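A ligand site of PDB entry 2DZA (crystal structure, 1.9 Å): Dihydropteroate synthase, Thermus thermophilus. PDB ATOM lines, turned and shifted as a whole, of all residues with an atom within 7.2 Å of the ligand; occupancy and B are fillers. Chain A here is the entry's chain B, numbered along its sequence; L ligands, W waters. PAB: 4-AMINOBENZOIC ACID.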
ATOM      1  N   SER A  75       4.438  11.516  22.772  1.00  0.00           N
ATOM      2  CA  SER A  75       5.702  11.597  22.044  1.00  0.00           C
ATOM      3  C   SER A  75       6.880  11.973  22.937  1.00  0.00           C
ATOM      4  O   SER A  75       6.860  12.940  23.685  1.00  0.00           O
ATOM      5  CB  SER A  75       5.553  12.652  20.955  1.00  0.00           C
ATOM      6  OG  SER A  75       6.779  12.762  20.243  1.00  0.00           O
ATOM      7  N   THR A  76       7.954  11.154  22.838  1.00  0.00           N
ATOM      8  CA  THR A  76       9.178  11.458  23.561  1.00  0.00           C
ATOM      9  C   THR A  76      10.264  12.000  22.634  1.00  0.00           C
ATOM     10  O   THR A  76      11.442  12.073  22.965  1.00  0.00           O
ATOM     11  CB  THR A  76       9.662  10.164  24.234  1.00  0.00           C
ATOM     12  OG1 THR A  76       9.993   9.221  23.211  1.00  0.00           O
ATOM     13  CG2 THR A  76       8.540   9.586  25.095  1.00  0.00           C
ATOM     14  N   ARG A  77       9.830  12.342  21.403  1.00  0.00           N
ATOM     15  CA  ARG A  77      10.763  12.899  20.422  1.00  0.00           C
ATOM     16  C   ARG A  77      11.487  14.125  20.982  1.00  0.00           C
ATOM     17  O   ARG A  77      10.982  14.864  21.805  1.00  0.00           O
ATOM     18  CB  ARG A  77       9.932  13.310  19.197  1.00  0.00           C
ATOM     19  CG  ARG A  77      10.807  13.752  18.024  1.00  0.00           C
ATOM     20  CD  ARG A  77      11.001  12.624  16.997  1.00  0.00           C
ATOM     21  NE  ARG A  77      12.260  12.805  16.258  1.00  0.00           N
ATOM     22  CZ  ARG A  77      12.324  13.825  15.377  1.00  0.00           C
ATOM     23  NH1 ARG A  77      11.301  14.641  15.227  1.00  0.00           N
ATOM     24  NH2 ARG A  77      13.419  13.971  14.620  1.00  0.00           N
ATOM     25  N   PRO A  78      12.730  14.305  20.542  1.00  0.00           N
ATOM     26  CA  PRO A  78      13.535  15.431  21.017  1.00  0.00           C
ATOM     27  C   PRO A  78      13.022  16.783  20.525  1.00  0.00           C
ATOM     28  O   PRO A  78      12.296  17.499  21.214  1.00  0.00           O
ATOM     29  CB  PRO A  78      14.941  15.195  20.454  1.00  0.00           C
ATOM     30  CG  PRO A  78      14.733  14.431  19.159  1.00  0.00           C
ATOM     31  CD  PRO A  78      13.495  13.510  19.611  1.00  0.00           C
ATOM     32  N   VAL A 130      10.360   6.051  29.870  1.00  0.00           N
ATOM     33  CA  VAL A 130      11.468   6.833  29.319  1.00  0.00           C
ATOM     34  C   VAL A 130      12.232   7.631  30.375  1.00  0.00           C
ATOM     35  O   VAL A 130      13.410   7.945  30.190  1.00  0.00           O
ATOM     36  CB  VAL A 130      10.984   7.807  28.213  1.00  0.00           C
ATOM     37  CG1 VAL A 130      10.830   7.059  26.900  1.00  0.00           C
ATOM     38  CG2 VAL A 130       9.663   8.443  28.622  1.00  0.00           C
ATOM     39  N   PRO A 159      12.048  15.356  27.756  1.00  0.00           N
ATOM     40  CA  PRO A 159      12.404  15.204  26.333  1.00  0.00           C
ATOM     41  C   PRO A 159      12.555  16.529  25.592  1.00  0.00           C
ATOM     42  O   PRO A 159      13.208  16.595  24.544  1.00  0.00           O
ATOM     43  CB  PRO A 159      11.245  14.373  25.780  1.00  0.00           C
ATOM     44  CG  PRO A 159      10.781  13.593  26.975  1.00  0.00           C
ATOM     45  CD  PRO A 159      10.793  14.645  28.050  1.00  0.00           C
ATOM     46  N   MET A 162      16.159  17.489  26.845  1.00  0.00           N
ATOM     47  CA  MET A 162      17.161  16.425  26.907  1.00  0.00           C
ATOM     48  C   MET A 162      18.329  16.692  25.957  1.00  0.00           C
ATOM     49  O   MET A 162      19.481  16.578  26.354  1.00  0.00           O
ATOM     50  CB  MET A 162      16.528  15.060  26.586  1.00  0.00           C
ATOM     51  CG  MET A 162      16.156  14.849  25.135  1.00  0.00           C
ATOM     52  SD  MET A 162      15.488  13.198  24.887  1.00  0.00           S
ATOM     53  CE  MET A 162      14.066  13.532  23.872  1.00  0.00           C
ATOM     54  N   MET A 163      18.021  17.063  24.722  1.00  0.00           N
ATOM     55  CA  MET A 163      19.082  17.328  23.751  1.00  0.00           C
ATOM     56  C   MET A 163      19.948  18.509  24.200  1.00  0.00           C
ATOM     57  O   MET A 163      21.074  18.694  23.778  1.00  0.00           O
ATOM     58  CB  MET A 163      18.444  17.634  22.396  1.00  0.00           C
ATOM     59  CG  MET A 163      17.834  16.409  21.719  1.00  0.00           C
ATOM     60  SD  MET A 163      18.920  14.976  21.733  1.00  0.00           S
ATOM     61  CE  MET A 163      19.995  15.463  20.381  1.00  0.00           C
ATOM     62  N   GLY A 199      18.866   4.031  25.577  1.00  0.00           N
ATOM     63  CA  GLY A 199      18.195   5.249  25.145  1.00  0.00           C
ATOM     64  C   GLY A 199      18.914   6.005  24.055  1.00  0.00           C
ATOM     65  O   GLY A 199      19.205   7.190  24.199  1.00  0.00           O
ATOM     66  N   PHE A 200      19.198   5.324  22.947  1.00  0.00           N
ATOM     67  CA  PHE A 200      19.883   5.963  21.839  1.00  0.00           C
ATOM     68  C   PHE A 200      19.094   7.173  21.352  1.00  0.00           C
ATOM     69  O   PHE A 200      17.876   7.113  21.218  1.00  0.00           O
ATOM     70  CB  PHE A 200      20.071   4.975  20.687  1.00  0.00           C
ATOM     71  CG  PHE A 200      21.054   3.880  20.977  1.00  0.00           C
ATOM     72  CD1 PHE A 200      22.419   4.140  20.975  1.00  0.00           C
ATOM     73  CD2 PHE A 200      20.611   2.593  21.275  1.00  0.00           C
ATOM     74  CE1 PHE A 200      23.341   3.142  21.265  1.00  0.00           C
ATOM     75  CE2 PHE A 200      21.522   1.585  21.567  1.00  0.00           C
ATOM     76  CZ  PHE A 200      22.890   1.861  21.565  1.00  0.00           C
ATOM     77  N   GLY A 201      19.795   8.272  21.125  1.00  0.00           N
ATOM     78  CA  GLY A 201      19.149   9.480  20.659  1.00  0.00           C
ATOM     79  C   GLY A 201      18.575  10.360  21.753  1.00  0.00           C
ATOM     80  O   GLY A 201      18.265  11.528  21.503  1.00  0.00           O
ATOM     81  N   PHE A 202      18.442   9.830  22.963  1.00  0.00           N
ATOM     82  CA  PHE A 202      17.887  10.596  24.065  1.00  0.00           C
ATOM     83  C   PHE A 202      18.965  11.388  24.800  1.00  0.00           C
ATOM     84  O   PHE A 202      19.636  10.863  25.688  1.00  0.00           O
ATOM     85  CB  PHE A 202      17.152   9.690  25.047  1.00  0.00           C
ATOM     86  CG  PHE A 202      15.861   9.140  24.513  1.00  0.00           C
ATOM     87  CD1 PHE A 202      15.839   7.993  23.728  1.00  0.00           C
ATOM     88  CD2 PHE A 202      14.657   9.782  24.796  1.00  0.00           C
ATOM     89  CE1 PHE A 202      14.638   7.484  23.233  1.00  0.00           C
ATOM     90  CE2 PHE A 202      13.450   9.279  24.303  1.00  0.00           C
ATOM     91  CZ  PHE A 202      13.440   8.130  23.522  1.00  0.00           C
ATOM     92  N   GLY A 203      19.107  12.659  24.428  1.00  0.00           N
ATOM     93  CA  GLY A 203      20.130  13.493  25.054  1.00  0.00           C
ATOM     94  C   GLY A 203      21.495  12.967  24.674  1.00  0.00           C
ATOM     95  O   GLY A 203      22.421  12.971  25.491  1.00  0.00           O
ATOM     96  N   LYS A 204      21.624  12.494  23.437  1.00  0.00           N
ATOM     97  CA  LYS A 204      22.881  11.942  22.943  1.00  0.00           C
ATOM     98  C   LYS A 204      23.130  12.313  21.495  1.00  0.00           C
ATOM     99  O   LYS A 204      22.240  12.194  20.654  1.00  0.00           O
ATOM    100  CB  LYS A 204      22.859  10.419  23.067  1.00  0.00           C
ATOM    101  CG  LYS A 204      22.688   9.914  24.495  1.00  0.00           C
ATOM    102  CD  LYS A 204      22.586   8.383  24.542  1.00  0.00           C
ATOM    103  CE  LYS A 204      22.237   7.892  25.943  1.00  0.00           C
ATOM    104  NZ  LYS A 204      20.842   8.218  26.354  1.00  0.00           N
ATOM    105  N   ASN A 209      26.082   8.029  20.716  1.00  0.00           N
ATOM    106  CA  ASN A 209      25.387   6.818  20.281  1.00  0.00           C
ATOM    107  C   ASN A 209      26.389   5.795  19.744  1.00  0.00           C
ATOM    108  O   ASN A 209      26.269   4.601  20.012  1.00  0.00           O
ATOM    109  CB  ASN A 209      24.331   7.146  19.224  1.00  0.00           C
ATOM    110  CG  ASN A 209      23.211   7.999  19.776  1.00  0.00           C
ATOM    111  OD1 ASN A 209      22.677   7.730  20.851  1.00  0.00           O
ATOM    112  ND2 ASN A 209      22.843   9.036  19.029  1.00  0.00           N
ATOM    113  N   GLY A 229      16.561   0.453  20.532  1.00  0.00           N
ATOM    114  CA  GLY A 229      15.707   0.898  19.435  1.00  0.00           C
ATOM    115  C   GLY A 229      16.355   2.076  18.715  1.00  0.00           C
ATOM    116  O   GLY A 229      16.455   3.192  19.231  1.00  0.00           O
ATOM    117  N   LEU A 230      16.859   1.794  17.497  1.00  0.00           N
ATOM    118  CA  LEU A 230      17.399   2.870  16.675  1.00  0.00           C
ATOM    119  C   LEU A 230      16.555   3.101  15.413  1.00  0.00           C
ATOM    120  O   LEU A 230      16.916   3.876  14.529  1.00  0.00           O
ATOM    121  CB  LEU A 230      18.826   2.499  16.286  1.00  0.00           C
ATOM    122  CG  LEU A 230      19.758   2.371  17.489  1.00  0.00           C
ATOM    123  CD1 LEU A 230      19.656   0.986  18.146  1.00  0.00           C
ATOM    124  CD2 LEU A 230      21.228   2.565  17.117  1.00  0.00           C
ATOM    125  N   SER A 231      15.426   2.381  15.318  1.00  0.00           N
ATOM    126  CA  SER A 231      14.585   2.496  14.132  1.00  0.00           C
ATOM    127  C   SER A 231      14.341   3.957  13.738  1.00  0.00           C
ATOM    128  O   SER A 231      13.796   4.759  14.484  1.00  0.00           O
ATOM    129  CB  SER A 231      13.251   1.797  14.400  1.00  0.00           C
ATOM    130  OG  SER A 231      13.434   0.388  14.317  1.00  0.00           O
ATOM    131  N   ARG A 232      14.806   4.293  12.511  1.00  0.00           N
ATOM    132  CA  ARG A 232      14.572   5.610  11.909  1.00  0.00           C
ATOM    133  C   ARG A 232      15.144   6.801  12.688  1.00  0.00           C
ATOM    134  O   ARG A 232      14.797   7.944  12.380  1.00  0.00           O
ATOM    135  CB  ARG A 232      13.092   5.820  11.706  1.00  0.00           C
ATOM    136  CG  ARG A 232      12.464   4.689  10.919  1.00  0.00           C
ATOM    137  CD  ARG A 232      10.953   4.915  10.701  1.00  0.00           C
ATOM    138  NE  ARG A 232      10.474   3.855   9.833  1.00  0.00           N
ATOM    139  CZ  ARG A 232       9.214   3.914   9.327  1.00  0.00           C
ATOM    140  NH1 ARG A 232       8.404   4.931   9.621  1.00  0.00           N
ATOM    141  NH2 ARG A 232       8.796   2.928   8.535  1.00  0.00           N
ATOM    142  N   LYS A 233      16.018   6.568  13.655  1.00  0.00           N
ATOM    143  CA  LYS A 233      16.577   7.673  14.434  1.00  0.00           C
ATOM    144  C   LYS A 233      17.599   8.518  13.672  1.00  0.00           C
ATOM    145  O   LYS A 233      18.153   8.097  12.650  1.00  0.00           O
ATOM    146  CB  LYS A 233      17.175   7.145  15.750  1.00  0.00           C
ATOM    147  CG  LYS A 233      16.126   6.534  16.696  1.00  0.00           C
ATOM    148  CD  LYS A 233      16.499   6.757  18.169  1.00  0.00           C
ATOM    149  CE  LYS A 233      15.564   6.001  19.117  1.00  0.00           C
ATOM    150  NZ  LYS A 233      14.152   6.340  18.852  1.00  0.00           N
ATOM    151  N   ARG A 234      17.844   9.730  14.173  1.00  0.00           N
ATOM    152  CA  ARG A 234      18.774  10.652  13.541  1.00  0.00           C
ATOM    153  C   ARG A 234      20.143  10.023  13.310  1.00  0.00           C
ATOM    154  O   ARG A 234      20.764  10.257  12.273  1.00  0.00           O
ATOM    155  CB  ARG A 234      18.949  11.912  14.390  1.00  0.00           C
ATOM    156  CG  ARG A 234      19.831  12.958  13.705  1.00  0.00           C
ATOM    157  CD  ARG A 234      20.168  14.155  14.606  1.00  0.00           C
ATOM    158  NE  ARG A 234      18.985  14.853  15.103  1.00  0.00           N
ATOM    159  CZ  ARG A 234      18.938  16.152  15.385  1.00  0.00           C
ATOM    160  NH1 ARG A 234      20.016  16.912  15.217  1.00  0.00           N
ATOM    161  NH2 ARG A 234      17.817  16.690  15.851  1.00  0.00           N
ATOM    162  N   THR A 235      20.635   9.238  14.267  1.00  0.00           N
ATOM    163  CA  THR A 235      21.942   8.601  14.107  1.00  0.00           C
ATOM    164  C   THR A 235      21.973   7.739  12.846  1.00  0.00           C
ATOM    165  O   THR A 235      22.981   7.711  12.141  1.00  0.00           O
ATOM    166  CB  THR A 235      22.307   7.737  15.327  1.00  0.00           C
ATOM    167  OG1 THR A 235      22.754   8.587  16.386  1.00  0.00           O
ATOM    168  CG2 THR A 235      23.425   6.746  14.976  1.00  0.00           C
ATOM    169  N   ILE A 236      20.879   7.041  12.564  1.00  0.00           N
ATOM    170  CA  ILE A 236      20.817   6.199  11.367  1.00  0.00           C
ATOM    171  C   ILE A 236      20.869   7.090  10.124  1.00  0.00           C
ATOM    172  O   ILE A 236      21.546   6.786   9.143  1.00  0.00           O
ATOM    173  CB  ILE A 236      19.531   5.351  11.375  1.00  0.00           C
ATOM    174  CG1 ILE A 236      19.492   4.470  12.630  1.00  0.00           C
ATOM    175  CG2 ILE A 236      19.469   4.479  10.119  1.00  0.00           C
ATOM    176  CD1 ILE A 236      20.679   3.520  12.771  1.00  0.00           C
ATOM    177  N   ARG A 248      14.635   4.873   6.372  1.00  0.00           N
ATOM    178  CA  ARG A 248      15.857   4.430   7.037  1.00  0.00           C
ATOM    179  C   ARG A 248      15.893   2.965   7.468  1.00  0.00           C
ATOM    180  O   ARG A 248      16.694   2.596   8.325  1.00  0.00           O
ATOM    181  CB  ARG A 248      16.113   5.321   8.259  1.00  0.00           C
ATOM    182  CG  ARG A 248      16.446   6.774   7.886  1.00  0.00           C
ATOM    183  CD  ARG A 248      16.541   7.705   9.093  1.00  0.00           C
ATOM    184  NE  ARG A 248      16.736   9.091   8.655  1.00  0.00           N
ATOM    185  CZ  ARG A 248      16.629  10.163   9.437  1.00  0.00           C
ATOM    186  NH1 ARG A 248      16.312  10.039  10.716  1.00  0.00           N
ATOM    187  NH2 ARG A 248      16.796  11.377   8.921  1.00  0.00           N
ATOM    188  N   ARG A 268      13.290  -2.769  19.515  1.00  0.00           N
ATOM    189  CA  ARG A 268      12.081  -1.950  19.340  1.00  0.00           C
ATOM    190  C   ARG A 268      12.151  -1.472  17.889  1.00  0.00           C
ATOM    191  O   ARG A 268      13.051  -0.706  17.534  1.00  0.00           O
ATOM    192  CB  ARG A 268      12.122  -0.752  20.296  1.00  0.00           C
ATOM    193  CG  ARG A 268      10.882   0.137  20.244  1.00  0.00           C
ATOM    194  CD  ARG A 268      10.865   1.118  21.425  1.00  0.00           C
ATOM    195  NE  ARG A 268       9.707   2.013  21.400  1.00  0.00           N
ATOM    196  CZ  ARG A 268       9.581   3.056  20.581  1.00  0.00           C
ATOM    197  NH1 ARG A 268      10.532   3.343  19.707  1.00  0.00           N
ATOM    198  NH2 ARG A 268       8.487   3.819  20.648  1.00  0.00           N
HETATM  199  C1' PAB L   1      16.201  10.344  17.361  1.00  0.00           C
HETATM  200  O1' PAB L   1      16.152  10.398  16.136  1.00  0.00           O
HETATM  201  O2' PAB L   1      17.334  10.501  17.818  1.00  0.00           O
HETATM  202  C1  PAB L   1      15.056  10.136  18.220  1.00  0.00           C
HETATM  203  C2  PAB L   1      13.733   9.942  17.708  1.00  0.00           C
HETATM  204  C3  PAB L   1      12.626   9.735  18.545  1.00  0.00           C
HETATM  205  C4  PAB L   1      12.814   9.709  19.950  1.00  0.00           C
HETATM  206  C5  PAB L   1      14.104   9.891  20.491  1.00  0.00           C
HETATM  207  C6  PAB L   1      15.208  10.099  19.640  1.00  0.00           C
HETATM  208  N4  PAB L   1      11.823   9.515  20.807  1.00  0.00           N
HETATM  209  O   HOH W   1      11.859   6.598  20.665  1.00  0.00           O
HETATM  210  O   HOH W   2      18.774  12.416  18.891  1.00  0.00           O
HETATM  211  O   HOH W   3      19.692   9.598  17.156  1.00  0.00           O
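OG1 of Thr 76 lies within hydrogen-bond range of N4 of the ligand (3.0 Å).
The backbone NH (N) of Arg 234 is in hydrogen-bond range of an oxygen (O1') of the ligand (2.7 Å).
The backbone carbonyl oxygen (O) of Thr 76 lies within hydrogen-bond range of a nitrogen (N4) of the ligand (3.4 Å).
Merely in contact with the ligand: Arg 77 (3.5 Å), Pro 78 (3.8 Å), Gly 201 (3.5 Å), Phe 202 (3.5 Å) and Lys 233 (3.2 Å).
Hydrophobic or aromatic side chains that line the ligand: Pro 78 and Phe 202.
Of the 25 residues printed, 7 come within 4 Å of the ligand.
The nearest printed residue that does not touch the ligand is Phe 200 (4.3 Å).
The backbone carbonyl oxygen (O) of Lys 233 is in hydrogen-bond range of the guanidinium group (NH1) of Arg 248, at 3.3 Å.
The backbone carbonyl oxygen (O) of Phe 202 lies within hydrogen-bond range of the side-chain amino group (NZ) of Lys 204 (3.0 Å).
The side-chain hydroxyl of Ser 75 lies within hydrogen-bond range of the backbone NH of Arg 77 (3.3 Å).
OD1 of Asn 209 lies within hydrogen-bond range of N of Gly 201 (2.9 Å).
Water W3 bridges an oxygen (O2') of the ligand (2.6 Å) and the backbone NH of Thr 235 (3.1 Å).
Water W2 lies within hydrogen-bond range of O2' of the ligand (2.6 Å) and O of Gly 201 (2.8 Å).
Water W1 bridges a nitrogen (N4) of the ligand (2.9 Å) and the side-chain amino group of Lys 233 (2.9 Å).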
